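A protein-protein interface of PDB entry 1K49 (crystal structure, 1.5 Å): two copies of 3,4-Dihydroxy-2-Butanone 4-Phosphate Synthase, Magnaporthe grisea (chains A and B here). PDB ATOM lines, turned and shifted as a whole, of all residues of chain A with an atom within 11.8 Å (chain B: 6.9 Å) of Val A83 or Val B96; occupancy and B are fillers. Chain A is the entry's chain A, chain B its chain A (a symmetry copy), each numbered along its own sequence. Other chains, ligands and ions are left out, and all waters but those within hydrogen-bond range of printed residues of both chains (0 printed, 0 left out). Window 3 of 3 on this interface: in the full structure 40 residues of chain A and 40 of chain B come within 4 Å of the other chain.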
ATOM      1  N   LEU A  64      -5.695   4.535  28.671  1.00  0.00           N
ATOM      2  CA  LEU A  64      -4.734   4.303  27.591  1.00  0.00           C
ATOM      3  C   LEU A  64      -3.851   3.127  28.105  1.00  0.00           C
ATOM      4  O   LEU A  64      -2.895   3.279  28.861  1.00  0.00           O
ATOM      5  CB  LEU A  64      -3.902   5.539  27.303  1.00  0.00           C
ATOM      6  CG  LEU A  64      -2.922   5.365  26.150  1.00  0.00           C
ATOM      7  CD1 LEU A  64      -3.680   5.114  24.856  1.00  0.00           C
ATOM      8  CD2 LEU A  64      -2.213   6.700  25.996  1.00  0.00           C
ATOM      9  N   THR A  74       9.885  -6.802  20.373  1.00  0.00           N
ATOM     10  CA  THR A  74       9.495  -5.937  19.240  1.00  0.00           C
ATOM     11  C   THR A  74      10.020  -6.471  17.896  1.00  0.00           C
ATOM     12  O   THR A  74       9.374  -6.377  16.850  1.00  0.00           O
ATOM     13  CB  THR A  74       9.862  -4.448  19.412  1.00  0.00           C
ATOM     14  OG1 THR A  74      11.256  -4.333  19.610  1.00  0.00           O
ATOM     15  CG2 THR A  74       9.100  -3.943  20.655  1.00  0.00           C
ATOM     16  N   LEU A  79       7.050  -5.272  15.569  1.00  0.00           N
ATOM     17  CA  LEU A  79       6.400  -4.105  16.120  1.00  0.00           C
ATOM     18  C   LEU A  79       7.304  -2.925  16.037  1.00  0.00           C
ATOM     19  O   LEU A  79       7.976  -2.541  16.962  1.00  0.00           O
ATOM     20  CB  LEU A  79       5.962  -4.351  17.579  1.00  0.00           C
ATOM     21  CG  LEU A  79       4.972  -5.503  17.706  1.00  0.00           C
ATOM     22  CD1 LEU A  79       4.810  -5.789  19.214  1.00  0.00           C
ATOM     23  CD2 LEU A  79       3.634  -5.120  17.079  1.00  0.00           C
ATOM     24  N   PRO A  80       7.383  -2.297  14.870  1.00  0.00           N
ATOM     25  CA  PRO A  80       8.269  -1.122  14.759  1.00  0.00           C
ATOM     26  C   PRO A  80       7.706   0.104  15.513  1.00  0.00           C
ATOM     27  O   PRO A  80       6.479   0.236  15.755  1.00  0.00           O
ATOM     28  CB  PRO A  80       8.297  -0.772  13.257  1.00  0.00           C
ATOM     29  CG  PRO A  80       6.999  -1.339  12.727  1.00  0.00           C
ATOM     30  CD  PRO A  80       6.621  -2.541  13.637  1.00  0.00           C
ATOM     31  N   GLN A  81       8.627   1.008  15.835  1.00  0.00           N
ATOM     32  CA  GLN A  81       8.260   2.254  16.497  1.00  0.00           C
ATOM     33  C   GLN A  81       7.218   3.035  15.688  1.00  0.00           C
ATOM     34  O   GLN A  81       7.208   3.089  14.457  1.00  0.00           O
ATOM     35  CB  GLN A  81       9.512   3.093  16.770  1.00  0.00           C
ATOM     36  CG  GLN A  81      10.377   2.463  17.901  1.00  0.00           C
ATOM     37  CD  GLN A  81       9.629   2.465  19.245  1.00  0.00           C
ATOM     38  OE1 GLN A  81       9.230   1.392  19.772  1.00  0.00           O
ATOM     39  NE2 GLN A  81       9.487   3.646  19.816  1.00  0.00           N
ATOM     40  N   MET A  82       6.274   3.632  16.403  1.00  0.00           N
ATOM     41  CA  MET A  82       5.223   4.405  15.754  1.00  0.00           C
ATOM     42  C   MET A  82       5.829   5.555  14.928  1.00  0.00           C
ATOM     43  O   MET A  82       5.336   5.897  13.823  1.00  0.00           O
ATOM     44  CB  MET A  82       4.363   5.017  16.889  1.00  0.00           C
ATOM     45  CG  MET A  82       3.012   5.363  16.324  1.00  0.00           C
ATOM     46  SD  MET A  82       1.979   6.279  17.494  1.00  0.00           S
ATOM     47  CE  MET A  82       1.409   4.853  18.464  1.00  0.00           C
ATOM     48  N   VAL A  83       6.815   6.162  15.531  1.00  0.00           N
ATOM     49  CA  VAL A  83       7.512   7.281  14.940  1.00  0.00           C
ATOM     50  C   VAL A  83       8.979   6.863  14.737  1.00  0.00           C
ATOM     51  O   VAL A  83       9.669   6.569  15.727  1.00  0.00           O
ATOM     52  CB  VAL A  83       7.351   8.534  15.816  1.00  0.00           C
ATOM     53  CG1 VAL A  83       8.299   9.665  15.447  1.00  0.00           C
ATOM     54  CG2 VAL A  83       5.917   9.031  15.754  1.00  0.00           C
ATOM     55  N   GLY A  91      12.024   9.409  25.830  1.00  0.00           N
ATOM     56  CA  GLY A  91      10.741   9.445  25.125  1.00  0.00           C
ATOM     57  C   GLY A  91      10.034   8.073  25.068  1.00  0.00           C
ATOM     58  O   GLY A  91      10.630   7.077  24.670  1.00  0.00           O
ATOM     59  N   THR A  92       8.762   8.012  25.462  1.00  0.00           N
ATOM     60  CA  THR A  92       7.991   6.772  25.463  1.00  0.00           C
ATOM     61  C   THR A  92       8.074   6.131  24.087  1.00  0.00           C
ATOM     62  O   THR A  92       7.731   6.725  23.054  1.00  0.00           O
ATOM     63  CB  THR A  92       6.523   7.012  25.906  1.00  0.00           C
ATOM     64  OG1 THR A  92       6.521   7.692  27.160  1.00  0.00           O
ATOM     65  CG2 THR A  92       5.749   5.693  26.001  1.00  0.00           C
ATOM     66  N   ALA A  93       8.567   4.898  24.099  1.00  0.00           N
ATOM     67  CA  ALA A  93       8.795   4.124  22.887  1.00  0.00           C
ATOM     68  C   ALA A  93       7.598   3.400  22.318  1.00  0.00           C
ATOM     69  O   ALA A  93       7.595   2.196  22.169  1.00  0.00           O
ATOM     70  CB  ALA A  93      10.003   3.227  23.181  1.00  0.00           C
ATOM     71  N   TYR A  94       6.494   4.117  21.956  1.00  0.00           N
ATOM     72  CA  TYR A  94       5.338   3.474  21.399  1.00  0.00           C
ATOM     73  C   TYR A  94       5.639   2.702  20.113  1.00  0.00           C
ATOM     74  O   TYR A  94       6.255   3.244  19.189  1.00  0.00           O
ATOM     75  CB  TYR A  94       4.287   4.511  20.959  1.00  0.00           C
ATOM     76  CG  TYR A  94       3.692   5.253  22.132  1.00  0.00           C
ATOM     77  CD1 TYR A  94       4.209   6.498  22.516  1.00  0.00           C
ATOM     78  CD2 TYR A  94       2.615   4.718  22.849  1.00  0.00           C
ATOM     79  CE1 TYR A  94       3.662   7.207  23.585  1.00  0.00           C
ATOM     80  CE2 TYR A  94       2.093   5.410  23.950  1.00  0.00           C
ATOM     81  CZ  TYR A  94       2.612   6.653  24.316  1.00  0.00           C
ATOM     82  OH  TYR A  94       2.077   7.324  25.399  1.00  0.00           O
ATOM     83  N   THR A  95       5.164   1.460  19.992  1.00  0.00           N
ATOM     84  CA  THR A  95       5.302   0.760  18.713  1.00  0.00           C
ATOM     85  C   THR A  95       3.976   0.996  17.973  1.00  0.00           C
ATOM     86  O   THR A  95       3.054   1.694  18.466  1.00  0.00           O
ATOM     87  CB  THR A  95       5.442  -0.779  18.878  1.00  0.00           C
ATOM     88  OG1 THR A  95       4.195  -1.329  19.258  1.00  0.00           O
ATOM     89  CG2 THR A  95       6.524  -1.141  19.920  1.00  0.00           C
ATOM     90  N   VAL A  96       3.820   0.386  16.796  1.00  0.00           N
ATOM     91  CA  VAL A  96       2.561   0.476  16.092  1.00  0.00           C
ATOM     92  C   VAL A  96       1.538  -0.195  17.058  1.00  0.00           C
ATOM     93  O   VAL A  96       1.960  -1.109  17.765  1.00  0.00           O
ATOM     94  CB  VAL A  96       2.641  -0.299  14.753  1.00  0.00           C
ATOM     95  CG1 VAL A  96       2.989  -1.768  14.998  1.00  0.00           C
ATOM     96  CG2 VAL A  96       1.332  -0.234  13.979  1.00  0.00           C
ATOM     97  N   SER A  97       0.269   0.276  17.142  1.00  0.00           N
ATOM     98  CA  SER A  97      -0.756  -0.289  18.047  1.00  0.00           C
ATOM     99  C   SER A  97      -1.309  -1.591  17.456  1.00  0.00           C
ATOM    100  O   SER A  97      -1.203  -1.898  16.245  1.00  0.00           O
ATOM    101  CB  SER A  97      -1.877   0.729  18.294  1.00  0.00           C
ATOM    102  OG  SER A  97      -2.375   1.091  17.020  1.00  0.00           O
ATOM    103  N   PRO A 134      -3.429  -1.097  12.564  1.00  0.00           N
ATOM    104  CA  PRO A 134      -3.252  -0.578  13.912  1.00  0.00           C
ATOM    105  C   PRO A 134      -4.401  -1.131  14.779  1.00  0.00           C
ATOM    106  O   PRO A 134      -5.239  -1.900  14.307  1.00  0.00           O
ATOM    107  CB  PRO A 134      -3.406   0.955  13.754  1.00  0.00           C
ATOM    108  CG  PRO A 134      -4.408   1.097  12.634  1.00  0.00           C
ATOM    109  CD  PRO A 134      -4.198  -0.121  11.707  1.00  0.00           C
ATOM    110  N   GLY A 135      -4.434  -0.766  16.054  1.00  0.00           N
ATOM    111  CA  GLY A 135      -5.479  -1.275  16.903  1.00  0.00           C
ATOM    112  C   GLY A 135      -5.605  -0.413  18.147  1.00  0.00           C
ATOM    113  O   GLY A 135      -5.233   0.791  18.165  1.00  0.00           O
ATOM    114  N   PHE A 138      -1.442  -0.507  23.064  1.00  0.00           N
ATOM    115  CA  PHE A 138      -0.203   0.209  22.740  1.00  0.00           C
ATOM    116  C   PHE A 138       1.048  -0.389  23.362  1.00  0.00           C
ATOM    117  O   PHE A 138       1.438  -0.046  24.477  1.00  0.00           O
ATOM    118  CB  PHE A 138      -0.360   1.712  23.163  1.00  0.00           C
ATOM    119  CG  PHE A 138      -1.544   2.268  22.402  1.00  0.00           C
ATOM    120  CD1 PHE A 138      -2.852   2.124  22.869  1.00  0.00           C
ATOM    121  CD2 PHE A 138      -1.368   2.878  21.157  1.00  0.00           C
ATOM    122  CE1 PHE A 138      -3.939   2.574  22.114  1.00  0.00           C
ATOM    123  CE2 PHE A 138      -2.447   3.349  20.403  1.00  0.00           C
ATOM    124  CZ  PHE A 138      -3.751   3.179  20.875  1.00  0.00           C
ATOM    125  N   PRO A 139       1.728  -1.260  22.562  1.00  0.00           N
ATOM    126  CA  PRO A 139       2.969  -1.831  23.087  1.00  0.00           C
ATOM    127  C   PRO A 139       4.009  -0.726  23.272  1.00  0.00           C
ATOM    128  O   PRO A 139       4.019   0.249  22.531  1.00  0.00           O
ATOM    129  CB  PRO A 139       3.391  -2.937  22.070  1.00  0.00           C
ATOM    130  CG  PRO A 139       2.168  -3.202  21.201  1.00  0.00           C
ATOM    131  CD  PRO A 139       1.316  -1.923  21.291  1.00  0.00           C
ATOM    132  N   LEU A 140       4.912  -0.855  24.242  1.00  0.00           N
ATOM    133  CA  LEU A 140       5.944   0.106  24.504  1.00  0.00           C
ATOM    134  C   LEU A 140       7.268  -0.674  24.625  1.00  0.00           C
ATOM    135  O   LEU A 140       7.388  -1.664  25.374  1.00  0.00           O
ATOM    136  CB  LEU A 140       5.732   0.861  25.832  1.00  0.00           C
ATOM    137  CG  LEU A 140       4.356   1.531  25.918  1.00  0.00           C
ATOM    138  CD1 LEU A 140       4.172   2.116  27.316  1.00  0.00           C
ATOM    139  CD2 LEU A 140       4.269   2.668  24.897  1.00  0.00           C
ATOM    140  N   ARG A 141       8.272  -0.167  23.913  1.00  0.00           N
ATOM    141  CA  ARG A 141       9.601  -0.764  23.869  1.00  0.00           C
ATOM    142  C   ARG A 141      10.491  -0.379  25.018  1.00  0.00           C
ATOM    143  O   ARG A 141      10.958   0.772  25.048  1.00  0.00           O
ATOM    144  CB  ARG A 141      10.304  -0.529  22.492  1.00  0.00           C
ATOM    145  CG  ARG A 141      11.663  -1.261  22.449  1.00  0.00           C
ATOM    146  CD  ARG A 141      12.414  -1.018  21.118  1.00  0.00           C
ATOM    147  NE  ARG A 141      12.759   0.380  21.087  1.00  0.00           N
ATOM    148  CZ  ARG A 141      13.055   1.019  19.986  1.00  0.00           C
ATOM    149  NH1 ARG A 141      13.133   0.359  18.823  1.00  0.00           N
ATOM    150  NH2 ARG A 141      13.316   2.314  20.117  1.00  0.00           N
ATOM    151  N   ASP B  78       0.062  17.941   9.160  1.00  0.00           N
ATOM    152  CA  ASP B  78       1.122  16.943   8.962  1.00  0.00           C
ATOM    153  C   ASP B  78       0.945  15.739   9.878  1.00  0.00           C
ATOM    154  O   ASP B  78       1.858  15.407  10.637  1.00  0.00           O
ATOM    155  CB  ASP B  78       2.512  17.526   9.230  1.00  0.00           C
ATOM    156  CG  ASP B  78       3.510  16.627   8.561  1.00  0.00           C
ATOM    157  OD1 ASP B  78       3.218  15.539   8.032  1.00  0.00           O
ATOM    158  OD2 ASP B  78       4.691  17.184   8.577  1.00  0.00           O
ATOM    159  N   LEU B  79      -0.244  15.148   9.764  1.00  0.00           N
ATOM    160  CA  LEU B  79      -0.621  13.993  10.545  1.00  0.00           C
ATOM    161  C   LEU B  79      -0.780  12.805   9.662  1.00  0.00           C
ATOM    162  O   LEU B  79      -1.848  12.425   9.250  1.00  0.00           O
ATOM    163  CB  LEU B  79      -1.920  14.259  11.335  1.00  0.00           C
ATOM    164  CG  LEU B  79      -1.782  15.420  12.313  1.00  0.00           C
ATOM    165  CD1 LEU B  79      -3.197  15.724  12.848  1.00  0.00           C
ATOM    166  CD2 LEU B  79      -0.840  15.041  13.452  1.00  0.00           C
ATOM    167  N   PRO B  80       0.324  12.164   9.297  1.00  0.00           N
ATOM    168  CA  PRO B  80       0.197  10.980   8.424  1.00  0.00           C
ATOM    169  C   PRO B  80      -0.400   9.767   9.173  1.00  0.00           C
ATOM    170  O   PRO B  80      -0.324   9.648  10.422  1.00  0.00           O
ATOM    171  CB  PRO B  80       1.640  10.614   8.021  1.00  0.00           C
ATOM    172  CG  PRO B  80       2.486  11.186   9.136  1.00  0.00           C
ATOM    173  CD  PRO B  80       1.712  12.401   9.719  1.00  0.00           C
ATOM    174  N   GLN B  81      -0.952   8.859   8.373  1.00  0.00           N
ATOM    175  CA  GLN B  81      -1.510   7.624   8.909  1.00  0.00           C
ATOM    176  C   GLN B  81      -0.470   6.842   9.721  1.00  0.00           C
ATOM    177  O   GLN B  81       0.723   6.775   9.420  1.00  0.00           O
ATOM    178  CB  GLN B  81      -2.098   6.777   7.777  1.00  0.00           C
ATOM    179  CG  GLN B  81      -3.406   7.412   7.219  1.00  0.00           C
ATOM    180  CD  GLN B  81      -4.517   7.431   8.283  1.00  0.00           C
ATOM    181  OE1 GLN B  81      -4.917   8.512   8.791  1.00  0.00           O
ATOM    182  NE2 GLN B  81      -5.043   6.257   8.578  1.00  0.00           N
ATOM    183  N   MET B  82      -0.927   6.261  10.822  1.00  0.00           N
ATOM    184  CA  MET B  82      -0.040   5.490  11.682  1.00  0.00           C
ATOM    185  C   MET B  82       0.597   4.326  10.900  1.00  0.00           C
ATOM    186  O   MET B  82       1.787   3.976  11.100  1.00  0.00           O
ATOM    187  CB  MET B  82      -0.924   4.897  12.808  1.00  0.00           C
ATOM    188  CG  MET B  82      -0.040   4.557  13.975  1.00  0.00           C
ATOM    189  SD  MET B  82      -0.917   3.662  15.282  1.00  0.00           S
ATOM    190  CE  MET B  82      -1.699   5.102  16.063  1.00  0.00           C
ATOM    191  N   VAL B  83      -0.242   3.717  10.105  1.00  0.00           N
ATOM    192  CA  VAL B  83       0.144   2.587   9.293  1.00  0.00           C
ATOM    193  C   VAL B  83      -0.027   2.990   7.818  1.00  0.00           C
ATOM    194  O   VAL B  83      -1.157   3.289   7.398  1.00  0.00           O
ATOM    195  CB  VAL B  83      -0.673   1.344   9.684  1.00  0.00           C
ATOM    196  CG1 VAL B  83      -0.566   0.202   8.686  1.00  0.00           C
ATOM    197  CG2 VAL B  83      -0.254   0.858  11.061  1.00  0.00           C
ATOM    198  N   ALA B  93      -8.963   5.059  10.566  1.00  0.00           N
ATOM    199  CA  ALA B  93      -7.842   5.818  10.030  1.00  0.00           C
ATOM    200  C   ALA B  93      -6.982   6.545  11.036  1.00  0.00           C
ATOM    201  O   ALA B  93      -6.828   7.748  10.988  1.00  0.00           O
ATOM    202  CB  ALA B  93      -8.425   6.707   8.927  1.00  0.00           C
ATOM    203  N   TYR B  94      -6.359   5.834  12.020  1.00  0.00           N
ATOM    204  CA  TYR B  94      -5.521   6.480  12.991  1.00  0.00           C
ATOM    205  C   TYR B  94      -4.348   7.236  12.365  1.00  0.00           C
ATOM    206  O   TYR B  94      -3.615   6.679  11.541  1.00  0.00           O
ATOM    207  CB  TYR B  94      -4.839   5.448  13.907  1.00  0.00           C
ATOM    208  CG  TYR B  94      -5.828   4.723  14.787  1.00  0.00           C
ATOM    209  CD1 TYR B  94      -6.342   3.478  14.398  1.00  0.00           C
ATOM    210  CD2 TYR B  94      -6.245   5.274  16.005  1.00  0.00           C
ATOM    211  CE1 TYR B  94      -7.243   2.785  15.206  1.00  0.00           C
ATOM    212  CE2 TYR B  94      -7.184   4.599  16.797  1.00  0.00           C
ATOM    213  CZ  TYR B  94      -7.680   3.355  16.401  1.00  0.00           C
ATOM    214  OH  TYR B  94      -8.598   2.701  17.199  1.00  0.00           O
ATOM    215  N   THR B  95      -4.100   8.480  12.780  1.00  0.00           N
ATOM    216  CA  THR B  95      -2.891   9.165  12.316  1.00  0.00           C
ATOM    217  C   THR B  95      -1.842   8.933  13.413  1.00  0.00           C
ATOM    218  O   THR B  95      -2.092   8.248  14.438  1.00  0.00           O
ATOM    219  CB  THR B  95      -3.074  10.705  12.206  1.00  0.00           C
ATOM    220  OG1 THR B  95      -3.121  11.270  13.503  1.00  0.00           O
ATOM    221  CG2 THR B  95      -4.354  11.069  11.420  1.00  0.00           C
ATOM    222  N   VAL B  96      -0.659   9.531  13.260  1.00  0.00           N
ATOM    223  CA  VAL B  96       0.340   9.444  14.301  1.00  0.00           C
ATOM    224  C   VAL B  96      -0.330  10.133  15.528  1.00  0.00           C
ATOM    225  O   VAL B  96      -1.112  11.052  15.288  1.00  0.00           O
ATOM    226  CB  VAL B  96       1.622  10.204  13.876  1.00  0.00           C
ATOM    227  CG1 VAL B  96       1.308  11.672  13.585  1.00  0.00           C
ATOM    228  CG2 VAL B  96       2.701  10.141  14.947  1.00  0.00           C
ATOM    229  N   SER B  97      -0.094   9.674  16.781  1.00  0.00           N
ATOM    230  CA  SER B  97      -0.704  10.257  17.997  1.00  0.00           C
ATOM    231  C   SER B  97       0.018  11.558  18.368  1.00  0.00           C
ATOM    232  O   SER B  97       1.165  11.850  17.955  1.00  0.00           O
ATOM    233  CB  SER B  97      -0.668   9.252  19.154  1.00  0.00           C
ATOM    234  OG  SER B  97       0.688   8.880  19.317  1.00  0.00           O
ATOM    235  N   VAL B  98      -0.603  12.349  19.221  1.00  0.00           N
ATOM    236  CA  VAL B  98       0.033  13.616  19.571  1.00  0.00           C
ATOM    237  C   VAL B  98      -0.217  14.042  21.006  1.00  0.00           C
ATOM    238  O   VAL B  98      -1.172  13.573  21.643  1.00  0.00           O
ATOM    239  CB  VAL B  98      -0.624  14.760  18.714  1.00  0.00           C
ATOM    240  CG1 VAL B  98      -0.437  14.583  17.192  1.00  0.00           C
ATOM    241  CG2 VAL B  98      -2.112  14.976  19.068  1.00  0.00           C
ATOM    242  N   ARG B 132       3.393  17.503  19.632  1.00  0.00           N
ATOM    243  CA  ARG B 132       4.519  16.618  19.868  1.00  0.00           C
ATOM    244  C   ARG B 132       4.075  15.246  19.338  1.00  0.00           C
ATOM    245  O   ARG B 132       2.916  14.859  19.514  1.00  0.00           O
ATOM    246  CB  ARG B 132       4.843  16.558  21.360  1.00  0.00           C
ATOM    247  CG  ARG B 132       4.811  17.980  21.876  1.00  0.00           C
ATOM    248  CD  ARG B 132       5.890  18.341  22.852  1.00  0.00           C
ATOM    249  NE  ARG B 132       5.509  18.085  24.220  1.00  0.00           N
ATOM    250  CZ  ARG B 132       5.472  18.936  25.236  1.00  0.00           C
ATOM    251  NH1 ARG B 132       5.754  20.245  25.186  1.00  0.00           N
ATOM    252  NH2 ARG B 132       5.121  18.387  26.380  1.00  0.00           N
ATOM    253  N   ARG B 133       4.965  14.501  18.691  1.00  0.00           N
ATOM    254  CA  ARG B 133       4.572  13.192  18.213  1.00  0.00           C
ATOM    255  C   ARG B 133       5.653  12.212  18.699  1.00  0.00           C
ATOM    256  O   ARG B 133       6.837  12.536  18.626  1.00  0.00           O
ATOM    257  CB  ARG B 133       4.469  13.106  16.679  1.00  0.00           C
ATOM    258  CG  ARG B 133       3.698  14.283  16.020  1.00  0.00           C
ATOM    259  CD  ARG B 133       4.586  15.545  15.709  1.00  0.00           C
ATOM    260  NE  ARG B 133       3.819  16.665  15.119  1.00  0.00           N
ATOM    261  CZ  ARG B 133       3.114  16.592  13.967  1.00  0.00           C
ATOM    262  NH1 ARG B 133       3.095  15.478  13.184  1.00  0.00           N
ATOM    263  NH2 ARG B 133       2.376  17.675  13.588  1.00  0.00           N
ATOM    264  N   PRO B 134       5.284  11.028  19.185  1.00  0.00           N
ATOM    265  CA  PRO B 134       3.930  10.523  19.361  1.00  0.00           C
ATOM    266  C   PRO B 134       3.387  11.094  20.686  1.00  0.00           C
ATOM    267  O   PRO B 134       4.062  11.865  21.369  1.00  0.00           O
ATOM    268  CB  PRO B 134       4.110   8.989  19.486  1.00  0.00           C
ATOM    269  CG  PRO B 134       5.445   8.844  20.173  1.00  0.00           C
ATOM    270  CD  PRO B 134       6.299  10.050  19.722  1.00  0.00           C
ATOM    271  N   GLY B 135       2.159  10.744  21.044  1.00  0.00           N
ATOM    272  CA  GLY B 135       1.607  11.270  22.265  1.00  0.00           C
ATOM    273  C   GLY B 135       0.428  10.423  22.711  1.00  0.00           C
ATOM    274  O   GLY B 135       0.306   9.216  22.368  1.00  0.00           O
ATOM    275  N   VAL B 137      -3.131  11.518  22.456  1.00  0.00           N
ATOM    276  CA  VAL B 137      -4.415  11.756  21.811  1.00  0.00           C
ATOM    277  C   VAL B 137      -4.322  11.173  20.406  1.00  0.00           C
ATOM    278  O   VAL B 137      -3.246  11.292  19.803  1.00  0.00           O
ATOM    279  CB  VAL B 137      -4.842  13.207  21.822  1.00  0.00           C
ATOM    280  CG1 VAL B 137      -6.094  13.305  20.971  1.00  0.00           C
ATOM    281  CG2 VAL B 137      -5.083  13.562  23.281  1.00  0.00           C
ATOM    282  N   PHE B 138      -5.382  10.535  19.928  1.00  0.00           N
ATOM    283  CA  PHE B 138      -5.388   9.806  18.655  1.00  0.00           C
ATOM    284  C   PHE B 138      -6.302  10.399  17.596  1.00  0.00           C
ATOM    285  O   PHE B 138      -7.482  10.065  17.505  1.00  0.00           O
ATOM    286  CB  PHE B 138      -5.770   8.309  18.930  1.00  0.00           C
ATOM    287  CG  PHE B 138      -4.739   7.754  19.888  1.00  0.00           C
ATOM    288  CD1 PHE B 138      -4.858   7.914  21.271  1.00  0.00           C
ATOM    289  CD2 PHE B 138      -3.584   7.129  19.410  1.00  0.00           C
ATOM    290  CE1 PHE B 138      -3.856   7.465  22.136  1.00  0.00           C
ATOM    291  CE2 PHE B 138      -2.586   6.659  20.268  1.00  0.00           C
ATOM    292  CZ  PHE B 138      -2.711   6.845  21.647  1.00  0.00           C
ATOM    293  N   PRO B 139      -5.693  11.256  16.726  1.00  0.00           N
ATOM    294  CA  PRO B 139      -6.511  11.823  15.653  1.00  0.00           C
ATOM    295  C   PRO B 139      -6.962  10.711  14.705  1.00  0.00           C
ATOM    296  O   PRO B 139      -6.256   9.728  14.518  1.00  0.00           O
ATOM    297  CB  PRO B 139      -5.625  12.915  14.975  1.00  0.00           C
ATOM    298  CG  PRO B 139      -4.472  13.180  15.935  1.00  0.00           C
ATOM    299  CD  PRO B 139      -4.354  11.910  16.796  1.00  0.00           C
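The backbone carbonyl oxygen (O) of Pro A80 lies within hydrogen-bond range of the backbone NH (N) of Val A96 (2.9 Å).
The backbone carbonyl oxygen (O) of Tyr A94 sits at hydrogen-bond distance from the backbone NH (N) of Met A82, at 2.8 Å.
The backbone carbonyl oxygen of Pro B80 sits at hydrogen-bond distance from the backbone NH of Val B96 (2.9 Å).
The side-chain amide nitrogen of Gln B81 lies within hydrogen-bond range of the backbone carbonyl oxygen of Tyr B94, 3.3 Å away.
N of Met B82 is in hydrogen-bond range of O of Tyr B94 (2.8 Å).
OG of Ser B97 lies within hydrogen-bond range of N of Gly B135 (2.9 Å).
Met A82 touches its own counterpart, Met B82.
Met A82 touches Ser B97, and with the chains exchanged Ser A97 touches Met B82.
Val A83 touches Val B96, and with the chains exchanged Val A96 touches Val B83.
Tyr A94 touches Gly B135, and with the chains exchanged Gly A135 touches Tyr B94.
Of the 13 pairs that touch across the chains among the printed residues, 12 have their exchanged pair printed and touching as well.
Among the printed residues, merely in contact across the chains: Phe A138 with Phe B138, Val A96 with Val B83, Val A83 with Val B96, Tyr A94 with Pro B134, Pro A134 with Tyr B94, Leu A64 with Phe B138, Met A82 with Met B82, Gly A135 with Tyr B94, Tyr A94 with Gly B135, Met A82 with Pro B134 and Pro A134 with Met B82.
SD of Met A82 is in hydrogen-bond range of OG of Ser B97 (3.4 Å).
The side-chain hydroxyl (OG) of Ser A97 sits at hydrogen-bond distance from the side-chain sulfur (SD) of Met B82.
Val A83 touches just one residue of chain B: Val B96.
Printed residues of chain B within 4 Å of Gly A135: Tyr B94.
No residue of chain A comes within 4 Å of Leu B79.
No residue of chain A comes within 4 Å of Pro B80.
No residue of chain A comes within 4 Å of Gln B81.
Ala B93 touches none of the printed residues of chain A.
Val B96 touches one residue of chain A.
Of chain A, only Met A82 comes within 4 Å of Ser B97.
No residue of chain A comes within 4 Å of Val B98.
Of chain A, only Tyr A94 (3.96 Å) comes within 4 Å of Gly B135.
Of the printed residues of chain A, Phe B138 touches Leu A64 and Phe A138.
No residue of chain A comes within 4 Å of Pro B139.
The nearest printed residue of chain B that does not touch Pro A134 is Val B83 (4.02 Å).
Of the 20 printed residues of chain A, 9 touch a printed residue of chain B.
Hydrophobic or aromatic side chains of chain A that line the printed part of chain B: Leu A64, Met A82, Val A83, Tyr A94, Val A96, Pro A134 and Phe A138.
Of the 19 printed residues of chain B, 8 touch a printed residue of chain A.
Hydrophobic or aromatic side chains of chain B within 4 Å of the printed part of chain A: Met B82, Val B83, Tyr B94, Val B96, Pro B134 and Phe B138.
Among the printed residues, no Asp or Glu carboxylate lies within 4 Å of a Lys or Arg side-chain nitrogen of the other chain.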
